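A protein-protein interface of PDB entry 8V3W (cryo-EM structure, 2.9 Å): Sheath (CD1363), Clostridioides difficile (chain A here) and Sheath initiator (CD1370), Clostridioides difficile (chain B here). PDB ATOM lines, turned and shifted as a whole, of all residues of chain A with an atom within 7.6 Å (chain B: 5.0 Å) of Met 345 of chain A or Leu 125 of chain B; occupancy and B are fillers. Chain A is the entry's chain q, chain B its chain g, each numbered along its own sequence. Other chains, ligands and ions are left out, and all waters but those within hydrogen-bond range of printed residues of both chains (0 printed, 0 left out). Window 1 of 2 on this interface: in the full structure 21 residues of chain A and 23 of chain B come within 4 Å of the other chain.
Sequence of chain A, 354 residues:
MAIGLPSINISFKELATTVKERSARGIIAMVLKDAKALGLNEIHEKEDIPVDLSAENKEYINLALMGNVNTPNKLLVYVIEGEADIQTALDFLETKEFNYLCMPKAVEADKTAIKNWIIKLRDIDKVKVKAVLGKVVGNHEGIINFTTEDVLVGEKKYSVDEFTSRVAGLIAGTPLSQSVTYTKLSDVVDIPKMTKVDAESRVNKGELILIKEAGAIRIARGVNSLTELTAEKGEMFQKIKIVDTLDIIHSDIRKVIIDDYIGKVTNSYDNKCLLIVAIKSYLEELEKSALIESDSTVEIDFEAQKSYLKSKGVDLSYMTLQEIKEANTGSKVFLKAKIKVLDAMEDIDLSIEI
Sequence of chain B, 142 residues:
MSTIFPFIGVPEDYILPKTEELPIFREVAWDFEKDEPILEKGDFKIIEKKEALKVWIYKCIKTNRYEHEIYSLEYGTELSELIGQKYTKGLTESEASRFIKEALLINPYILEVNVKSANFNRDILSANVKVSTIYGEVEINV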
ATOM      1  N   SER A 177       9.724  24.333  11.479  1.00  0.00           N
ATOM      2  CA  SER A 177       9.461  23.168  10.644  1.00  0.00           C
ATOM      3  C   SER A 177      10.350  21.990  11.012  1.00  0.00           C
ATOM      4  O   SER A 177       9.973  20.843  10.759  1.00  0.00           O
ATOM      5  CB  SER A 177       9.642  23.527   9.171  1.00  0.00           C
ATOM      6  OG  SER A 177      10.688  24.463   8.998  1.00  0.00           O
ATOM      7  N   GLN A 178      11.506  22.246  11.613  1.00  0.00           N
ATOM      8  CA  GLN A 178      12.431  21.213  12.039  1.00  0.00           C
ATOM      9  C   GLN A 178      12.203  20.877  13.508  1.00  0.00           C
ATOM     10  O   GLN A 178      11.266  21.359  14.147  1.00  0.00           O
ATOM     11  CB  GLN A 178      13.871  21.670  11.818  1.00  0.00           C
ATOM     12  CG  GLN A 178      14.341  21.618  10.396  1.00  0.00           C
ATOM     13  CD  GLN A 178      15.769  22.078  10.259  1.00  0.00           C
ATOM     14  OE1 GLN A 178      16.590  21.858  11.147  1.00  0.00           O
ATOM     15  NE2 GLN A 178      16.080  22.713   9.137  1.00  0.00           N
ATOM     16  N   SER A 179      13.076  20.035  14.052  1.00  0.00           N
ATOM     17  CA  SER A 179      13.189  19.824  15.485  1.00  0.00           C
ATOM     18  C   SER A 179      14.665  19.815  15.843  1.00  0.00           C
ATOM     19  O   SER A 179      15.520  19.512  15.008  1.00  0.00           O
ATOM     20  CB  SER A 179      12.523  18.521  15.937  1.00  0.00           C
ATOM     21  OG  SER A 179      13.451  17.455  15.967  1.00  0.00           O
ATOM     22  N   THR A 181      16.295  17.828  17.626  1.00  0.00           N
ATOM     23  CA  THR A 181      16.876  16.506  17.817  1.00  0.00           C
ATOM     24  C   THR A 181      17.935  16.203  16.762  1.00  0.00           C
ATOM     25  O   THR A 181      17.733  16.442  15.570  1.00  0.00           O
ATOM     26  CB  THR A 181      15.775  15.447  17.775  1.00  0.00           C
ATOM     27  OG1 THR A 181      14.890  15.635  18.884  1.00  0.00           O
ATOM     28  CG2 THR A 181      16.359  14.056  17.834  1.00  0.00           C
ATOM     29  N   ARG A 221      17.838  14.197  22.177  1.00  0.00           N
ATOM     30  CA  ARG A 221      16.433  14.347  21.840  1.00  0.00           C
ATOM     31  C   ARG A 221      15.907  15.661  22.394  1.00  0.00           C
ATOM     32  O   ARG A 221      16.335  16.119  23.456  1.00  0.00           O
ATOM     33  CB  ARG A 221      15.608  13.174  22.377  1.00  0.00           C
ATOM     34  CG  ARG A 221      14.222  13.083  21.784  1.00  0.00           C
ATOM     35  CD  ARG A 221      13.839  11.650  21.509  1.00  0.00           C
ATOM     36  NE  ARG A 221      12.756  11.553  20.541  1.00  0.00           N
ATOM     37  CZ  ARG A 221      12.231  10.414  20.117  1.00  0.00           C
ATOM     38  NH1 ARG A 221      12.664   9.246  20.560  1.00  0.00           N
ATOM     39  NH2 ARG A 221      11.244  10.446  19.228  1.00  0.00           N
ATOM     40  N   LYS A 241       9.120  21.216  20.181  1.00  0.00           N
ATOM     41  CA  LYS A 241       8.551  21.785  18.965  1.00  0.00           C
ATOM     42  C   LYS A 241       7.056  22.048  19.113  1.00  0.00           C
ATOM     43  O   LYS A 241       6.558  23.100  18.690  1.00  0.00           O
ATOM     44  CB  LYS A 241       8.829  20.853  17.788  1.00  0.00           C
ATOM     45  CG  LYS A 241       8.085  21.200  16.522  1.00  0.00           C
ATOM     46  CD  LYS A 241       8.380  20.205  15.423  1.00  0.00           C
ATOM     47  CE  LYS A 241       7.637  20.566  14.154  1.00  0.00           C
ATOM     48  NZ  LYS A 241       7.929  19.626  13.048  1.00  0.00           N
ATOM     49  N   ASP A 343       4.498  16.995  13.789  1.00  0.00           N
ATOM     50  CA  ASP A 343       5.738  16.724  14.497  1.00  0.00           C
ATOM     51  C   ASP A 343       6.801  16.287  13.499  1.00  0.00           C
ATOM     52  O   ASP A 343       6.496  15.782  12.417  1.00  0.00           O
ATOM     53  CB  ASP A 343       5.553  15.649  15.573  1.00  0.00           C
ATOM     54  CG  ASP A 343       6.553  15.783  16.705  1.00  0.00           C
ATOM     55  OD1 ASP A 343       7.558  16.496  16.530  1.00  0.00           O
ATOM     56  OD2 ASP A 343       6.333  15.174  17.771  1.00  0.00           O
ATOM     57  N   ALA A 344       8.058  16.496  13.875  1.00  0.00           N
ATOM     58  CA  ALA A 344       9.172  16.078  13.041  1.00  0.00           C
ATOM     59  C   ALA A 344       9.345  14.563  13.100  1.00  0.00           C
ATOM     60  O   ALA A 344       8.928  13.904  14.049  1.00  0.00           O
ATOM     61  CB  ALA A 344      10.458  16.768  13.485  1.00  0.00           C
ATOM     62  N   MET A 345       9.973  14.016  12.063  1.00  0.00           N
ATOM     63  CA  MET A 345      10.233  12.584  12.001  1.00  0.00           C
ATOM     64  C   MET A 345      11.487  12.244  12.792  1.00  0.00           C
ATOM     65  O   MET A 345      12.542  12.850  12.590  1.00  0.00           O
ATOM     66  CB  MET A 345      10.390  12.129  10.551  1.00  0.00           C
ATOM     67  CG  MET A 345      10.786  10.669  10.401  1.00  0.00           C
ATOM     68  SD  MET A 345      12.078  10.411   9.172  1.00  0.00           S
ATOM     69  CE  MET A 345      13.526  10.327  10.214  1.00  0.00           C
ATOM     70  N   GLU A 346      11.374  11.270  13.693  1.00  0.00           N
ATOM     71  CA  GLU A 346      12.497  10.896  14.539  1.00  0.00           C
ATOM     72  C   GLU A 346      12.687   9.394  14.696  1.00  0.00           C
ATOM     73  O   GLU A 346      13.611   8.985  15.402  1.00  0.00           O
ATOM     74  CB  GLU A 346      12.345  11.535  15.926  1.00  0.00           C
ATOM     75  CG  GLU A 346      12.525  13.040  15.928  1.00  0.00           C
ATOM     76  CD  GLU A 346      11.833  13.710  17.094  1.00  0.00           C
ATOM     77  OE1 GLU A 346      10.926  13.092  17.681  1.00  0.00           O
ATOM     78  OE2 GLU A 346      12.199  14.854  17.426  1.00  0.00           O
ATOM     79  N   ASP A 347      11.855   8.563  14.076  1.00  0.00           N
ATOM     80  CA  ASP A 347      12.007   7.118  14.143  1.00  0.00           C
ATOM     81  C   ASP A 347      11.669   6.517  12.787  1.00  0.00           C
ATOM     82  O   ASP A 347      10.901   7.092  12.013  1.00  0.00           O
ATOM     83  CB  ASP A 347      11.112   6.506  15.222  1.00  0.00           C
ATOM     84  CG  ASP A 347      11.558   6.865  16.621  1.00  0.00           C
ATOM     85  OD1 ASP A 347      12.756   6.692  16.924  1.00  0.00           O
ATOM     86  OD2 ASP A 347      10.714   7.318  17.421  1.00  0.00           O
ATOM     87  N   ILE A 348      12.249   5.354  12.506  1.00  0.00           N
ATOM     88  CA  ILE A 348      12.017   4.643  11.254  1.00  0.00           C
ATOM     89  C   ILE A 348      11.660   3.200  11.576  1.00  0.00           C
ATOM     90  O   ILE A 348      12.376   2.535  12.331  1.00  0.00           O
ATOM     91  CB  ILE A 348      13.243   4.701  10.325  1.00  0.00           C
ATOM     92  CG1 ILE A 348      13.541   6.144   9.924  1.00  0.00           C
ATOM     93  CG2 ILE A 348      13.009   3.867   9.088  1.00  0.00           C
ATOM     94  CD1 ILE A 348      14.863   6.317   9.237  1.00  0.00           C
ATOM     95  N   ASP A 349      10.557   2.720  11.005  1.00  0.00           N
ATOM     96  CA  ASP A 349      10.112   1.338  11.167  1.00  0.00           C
ATOM     97  C   ASP A 349      10.121   0.663   9.803  1.00  0.00           C
ATOM     98  O   ASP A 349       9.313   1.005   8.935  1.00  0.00           O
ATOM     99  CB  ASP A 349       8.721   1.279  11.792  1.00  0.00           C
ATOM    100  CG  ASP A 349       8.722   1.666  13.253  1.00  0.00           C
ATOM    101  OD1 ASP A 349       9.746   2.199  13.729  1.00  0.00           O
ATOM    102  OD2 ASP A 349       7.700   1.432  13.931  1.00  0.00           O
ATOM    103  N   LEU A 350      11.014  -0.302   9.621  1.00  0.00           N
ATOM    104  CA  LEU A 350      11.170  -1.002   8.354  1.00  0.00           C
ATOM    105  C   LEU A 350      10.581  -2.399   8.459  1.00  0.00           C
ATOM    106  O   LEU A 350      10.923  -3.156   9.371  1.00  0.00           O
ATOM    107  CB  LEU A 350      12.642  -1.089   7.952  1.00  0.00           C
ATOM    108  CG  LEU A 350      13.311   0.215   7.535  1.00  0.00           C
ATOM    109  CD1 LEU A 350      14.757  -0.031   7.169  1.00  0.00           C
ATOM    110  CD2 LEU A 350      12.561   0.838   6.377  1.00  0.00           C
ATOM    111  N   LEU B  82      18.536  11.956   8.188  1.00  0.00           N
ATOM    112  CA  LEU B  82      17.142  12.358   8.083  1.00  0.00           C
ATOM    113  C   LEU B  82      16.497  12.643   9.430  1.00  0.00           C
ATOM    114  O   LEU B  82      15.422  13.250   9.463  1.00  0.00           O
ATOM    115  CB  LEU B  82      16.337  11.273   7.366  1.00  0.00           C
ATOM    116  CG  LEU B  82      16.864  10.809   6.012  1.00  0.00           C
ATOM    117  CD1 LEU B  82      15.966   9.734   5.449  1.00  0.00           C
ATOM    118  CD2 LEU B  82      16.960  11.974   5.054  1.00  0.00           C
ATOM    119  N   ILE B  83      17.120  12.230  10.532  1.00  0.00           N
ATOM    120  CA  ILE B  83      16.503  12.363  11.844  1.00  0.00           C
ATOM    121  C   ILE B  83      16.383  13.836  12.206  1.00  0.00           C
ATOM    122  O   ILE B  83      17.362  14.589  12.151  1.00  0.00           O
ATOM    123  CB  ILE B  83      17.317  11.597  12.897  1.00  0.00           C
ATOM    124  CG1 ILE B  83      17.570  10.164  12.431  1.00  0.00           C
ATOM    125  CG2 ILE B  83      16.608  11.614  14.239  1.00  0.00           C
ATOM    126  CD1 ILE B  83      16.352   9.287  12.472  1.00  0.00           C
ATOM    127  N   GLY B  84      15.181  14.251  12.586  1.00  0.00           N
ATOM    128  CA  GLY B  84      14.927  15.622  12.959  1.00  0.00           C
ATOM    129  C   GLY B  84      14.302  16.485  11.890  1.00  0.00           C
ATOM    130  O   GLY B  84      14.191  17.698  12.091  1.00  0.00           O
ATOM    131  N   GLN B  85      13.895  15.902  10.762  1.00  0.00           N
ATOM    132  CA  GLN B  85      13.230  16.628   9.681  1.00  0.00           C
ATOM    133  C   GLN B  85      14.121  17.736   9.121  1.00  0.00           C
ATOM    134  O   GLN B  85      13.701  18.882   8.965  1.00  0.00           O
ATOM    135  CB  GLN B  85      11.883  17.188  10.144  1.00  0.00           C
ATOM    136  CG  GLN B  85      10.899  17.468   9.027  1.00  0.00           C
ATOM    137  CD  GLN B  85      10.219  16.216   8.526  1.00  0.00           C
ATOM    138  OE1 GLN B  85       9.393  15.628   9.217  1.00  0.00           O
ATOM    139  NE2 GLN B  85      10.568  15.798   7.320  1.00  0.00           N
ATOM    140  N   THR B  92      12.409  13.785   2.087  1.00  0.00           N
ATOM    141  CA  THR B  92      12.793  12.721   3.010  1.00  0.00           C
ATOM    142  C   THR B  92      12.405  11.352   2.468  1.00  0.00           C
ATOM    143  O   THR B  92      13.194  10.405   2.541  1.00  0.00           O
ATOM    144  CB  THR B  92      12.155  12.950   4.381  1.00  0.00           C
ATOM    145  OG1 THR B  92      12.536  14.237   4.875  1.00  0.00           O
ATOM    146  CG2 THR B  92      12.603  11.889   5.361  1.00  0.00           C
ATOM    147  N   GLU B  93      11.200  11.229   1.911  1.00  0.00           N
ATOM    148  CA  GLU B  93      10.782   9.954   1.333  1.00  0.00           C
ATOM    149  C   GLU B  93      11.699   9.538   0.187  1.00  0.00           C
ATOM    150  O   GLU B  93      12.158   8.385   0.121  1.00  0.00           O
ATOM    151  CB  GLU B  93       9.340  10.054   0.847  1.00  0.00           C
ATOM    152  CG  GLU B  93       8.305   9.773   1.908  1.00  0.00           C
ATOM    153  CD  GLU B  93       6.923   9.583   1.320  1.00  0.00           C
ATOM    154  OE1 GLU B  93       6.832   9.167   0.146  1.00  0.00           O
ATOM    155  OE2 GLU B  93       5.928   9.855   2.026  1.00  0.00           O
ATOM    156  N   ALA B  96      15.161   8.500   1.548  1.00  0.00           N
ATOM    157  CA  ALA B  96      15.144   7.221   2.249  1.00  0.00           C
ATOM    158  C   ALA B  96      15.114   6.061   1.266  1.00  0.00           C
ATOM    159  O   ALA B  96      15.880   5.092   1.401  1.00  0.00           O
ATOM    160  CB  ALA B  96      13.947   7.160   3.192  1.00  0.00           C
ATOM    161  N   ALA B 118       5.061   4.064   2.091  1.00  0.00           N
ATOM    162  CA  ALA B 118       5.719   5.079   2.910  1.00  0.00           C
ATOM    163  C   ALA B 118       4.650   5.940   3.560  1.00  0.00           C
ATOM    164  O   ALA B 118       3.817   6.520   2.859  1.00  0.00           O
ATOM    165  CB  ALA B 118       6.669   5.930   2.072  1.00  0.00           C
ATOM    166  N   ASN B 119       4.674   6.027   4.888  1.00  0.00           N
ATOM    167  CA  ASN B 119       3.643   6.720   5.646  1.00  0.00           C
ATOM    168  C   ASN B 119       4.278   7.521   6.771  1.00  0.00           C
ATOM    169  O   ASN B 119       5.286   7.104   7.346  1.00  0.00           O
ATOM    170  CB  ASN B 119       2.620   5.724   6.211  1.00  0.00           C
ATOM    171  CG  ASN B 119       1.528   6.398   7.019  1.00  0.00           C
ATOM    172  OD1 ASN B 119       0.847   7.302   6.534  1.00  0.00           O
ATOM    173  ND2 ASN B 119       1.344   5.947   8.254  1.00  0.00           N
ATOM    174  N   PHE B 120       3.688   8.673   7.078  1.00  0.00           N
ATOM    175  CA  PHE B 120       4.124   9.529   8.174  1.00  0.00           C
ATOM    176  C   PHE B 120       3.040   9.553   9.242  1.00  0.00           C
ATOM    177  O   PHE B 120       1.907   9.961   8.972  1.00  0.00           O
ATOM    178  CB  PHE B 120       4.417  10.947   7.688  1.00  0.00           C
ATOM    179  CG  PHE B 120       5.809  11.134   7.160  1.00  0.00           C
ATOM    180  CD1 PHE B 120       6.864  11.365   8.023  1.00  0.00           C
ATOM    181  CD2 PHE B 120       6.058  11.094   5.801  1.00  0.00           C
ATOM    182  CE1 PHE B 120       8.145  11.540   7.538  1.00  0.00           C
ATOM    183  CE2 PHE B 120       7.335  11.270   5.311  1.00  0.00           C
ATOM    184  CZ  PHE B 120       8.380  11.494   6.182  1.00  0.00           C
ATOM    185  N   ASP B 123       5.969  11.021  14.799  1.00  0.00           N
ATOM    186  CA  ASP B 123       7.386  11.119  14.492  1.00  0.00           C
ATOM    187  C   ASP B 123       7.949   9.839  13.893  1.00  0.00           C
ATOM    188  O   ASP B 123       9.169   9.654  13.897  1.00  0.00           O
ATOM    189  CB  ASP B 123       8.160  11.490  15.755  1.00  0.00           C
ATOM    190  CG  ASP B 123       7.763  10.652  16.941  1.00  0.00           C
ATOM    191  OD1 ASP B 123       6.691  10.019  16.882  1.00  0.00           O
ATOM    192  OD2 ASP B 123       8.514  10.631  17.934  1.00  0.00           O
ATOM    193  N   ILE B 124       7.098   8.948  13.396  1.00  0.00           N
ATOM    194  CA  ILE B 124       7.518   7.648  12.891  1.00  0.00           C
ATOM    195  C   ILE B 124       7.310   7.604  11.385  1.00  0.00           C
ATOM    196  O   ILE B 124       6.241   7.976  10.887  1.00  0.00           O
ATOM    197  CB  ILE B 124       6.755   6.508  13.583  1.00  0.00           C
ATOM    198  CG1 ILE B 124       6.921   6.606  15.096  1.00  0.00           C
ATOM    199  CG2 ILE B 124       7.252   5.168  13.088  1.00  0.00           C
ATOM    200  CD1 ILE B 124       5.932   5.772  15.867  1.00  0.00           C
ATOM    201  N   LEU B 125       8.328   7.146  10.663  1.00  0.00           N
ATOM    202  CA  LEU B 125       8.242   6.872   9.236  1.00  0.00           C
ATOM    203  C   LEU B 125       8.263   5.366   9.017  1.00  0.00           C
ATOM    204  O   LEU B 125       9.175   4.682   9.487  1.00  0.00           O
ATOM    205  CB  LEU B 125       9.397   7.533   8.482  1.00  0.00           C
ATOM    206  CG  LEU B 125       9.656   7.052   7.055  1.00  0.00           C
ATOM    207  CD1 LEU B 125       8.567   7.524   6.116  1.00  0.00           C
ATOM    208  CD2 LEU B 125      11.010   7.525   6.576  1.00  0.00           C
ATOM    209  N   SER B 126       7.262   4.857   8.307  1.00  0.00           N
ATOM    210  CA  SER B 126       7.134   3.435   8.030  1.00  0.00           C
ATOM    211  C   SER B 126       7.271   3.188   6.535  1.00  0.00           C
ATOM    212  O   SER B 126       6.907   4.036   5.719  1.00  0.00           O
ATOM    213  CB  SER B 126       5.790   2.899   8.517  1.00  0.00           C
ATOM    214  OG  SER B 126       5.511   3.346   9.829  1.00  0.00           O
ATOM    215  N   ALA B 127       7.799   2.020   6.178  1.00  0.00           N
ATOM    216  CA  ALA B 127       7.967   1.663   4.777  1.00  0.00           C
ATOM    217  C   ALA B 127       8.003   0.149   4.634  1.00  0.00           C
ATOM    218  O   ALA B 127       8.285  -0.577   5.588  1.00  0.00           O
ATOM    219  CB  ALA B 127       9.237   2.283   4.187  1.00  0.00           C
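O of Gly 84 of chain B lies within hydrogen-bond range of N of Ser 179 of chain A, 3.2 Å away.
The backbone carbonyl oxygen of Met 345 of chain A is in hydrogen-bond range of the backbone NH of Gly 84 of chain B, 3.0 Å away.
N of Met 345 of chain A lies within hydrogen-bond range of OE1 of Gln 85 of chain B (3.3 Å).
The guanidinium group (NH2) of Arg 221 of chain A lies within salt-bridge range of the side-chain carboxylate (OD2) of Asp 123 of chain B (3.0 Å).
O of Asp 123 of chain B lies within hydrogen-bond range of N of Glu 346 of chain A, 2.7 Å away.
N of Asp 347 of chain A is in hydrogen-bond range of O of Asp 123 of chain B, 2.9 Å away.
N of Leu 125 of chain B is in hydrogen-bond range of O of Asp 347 of chain A (2.9 Å).
The backbone carbonyl oxygen (O) of Leu 125 of chain B is in hydrogen-bond range of the backbone NH (N) of Asp 349 of chain A.
The backbone carbonyl oxygen of Asp 349 of chain A is in hydrogen-bond range of the backbone NH of Ala 127 of chain B (3.3 Å).
Among the printed residues, merely in contact across the chains: Ser 177 of chain A with Gln 85 of chain B (3.9 Å), Gln 178 of chain A with Gly 84 of chain B (3.9 Å), Gln 178 of chain A with Gln 85 of chain B (3.2 Å), Thr 181 of chain A with Ile 83 of chain B (3.9 Å), Thr 181 of chain A with Gly 84 of chain B (3.9 Å), Ala 344 of chain A with Gln 85 of chain B (3.7 Å), Ala 344 of chain A with Asp 123 of chain B (3.1 Å), Met 345 of chain A with Leu 82 of chain B (3.6 Å), Met 345 of chain A with Ile 83 of chain B (3.8 Å), Met 345 of chain A with Phe 120 of chain B (3.8 Å), Met 345 of chain A with Asp 123 of chain B (3.6 Å), Met 345 of chain A with Leu 125 of chain B (3.9 Å), Asp 347 of chain A with Ile 124 of chain B (3.5 Å), Ile 348 of chain A with Leu 125 of chain B (3.3 Å), Asp 349 of chain A with Ile 124 of chain B (3.8 Å) and Asp 349 of chain A with Ser 126 of chain B (3.4 Å).
Printed residues of chain B that touch a printed residue of chain A: Leu 82, Ile 83, Gly 84, Gln 85, Phe 120, Asp 123, Ile 124, Leu 125, Ser 126 and Ala 127.
Hydrophobic or aromatic side chains of chain B that line the printed part of chain A: Ile 83, Phe 120, Ile 124 and Leu 125.
Hydrophobic or aromatic side chains of chain A that line the printed part of chain B: Ala 344, Met 345 and Ile 348.
Printed residues of chain B within 4 Å of Gln 178 of chain A: Gly 84 (3.9 Å) and Gln 85 (3.2 Å).
Met 345 of chain A touches seven residues of chain B.
Of the printed residues of chain A, Gln 85 of chain B touches Ser 177, Gln 178, Ala 344 and Met 345.
Thr 92 of chain B touches none of the printed residues of chain A.
Glu 93 of chain B touches none of the printed residues of chain A.
Leu 125 of chain B touches four residues of chain A.
Of the printed residues of chain A, Ala 127 of chain B touches Asp 349 (3.3 Å).
The nearest residue of chain B that does not touch Met 345 of chain A is Thr 92 of chain B (4.1 Å).
The backbone carbonyl oxygen of Ser 126 of chain B sits at hydrogen-bond distance from the backbone NH of Asn 119 of chain B (3.1 Å).
The side-chain hydroxyl (OG) of Ser 179 of chain A sits close to the backbone NH (N) of Thr 181 of chain A, at 3.3 Å.
OG of Ser 179 of chain A lies within hydrogen-bond range of OE2 of Glu 346 of chain A.
The side-chain hydroxyl of Thr 181 of chain A lies within hydrogen-bond range of the side-chain carboxylate of Glu 346 of chain A, 3.2 Å away.
NH2 of Arg 221 of chain A lies within salt-bridge range of OE1 of Glu 346 of chain A (3.1 Å).
OD2 of Asp 347 of chain A is in salt-bridge range of NH2 of Arg 221 of chain A, 3.7 Å away.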
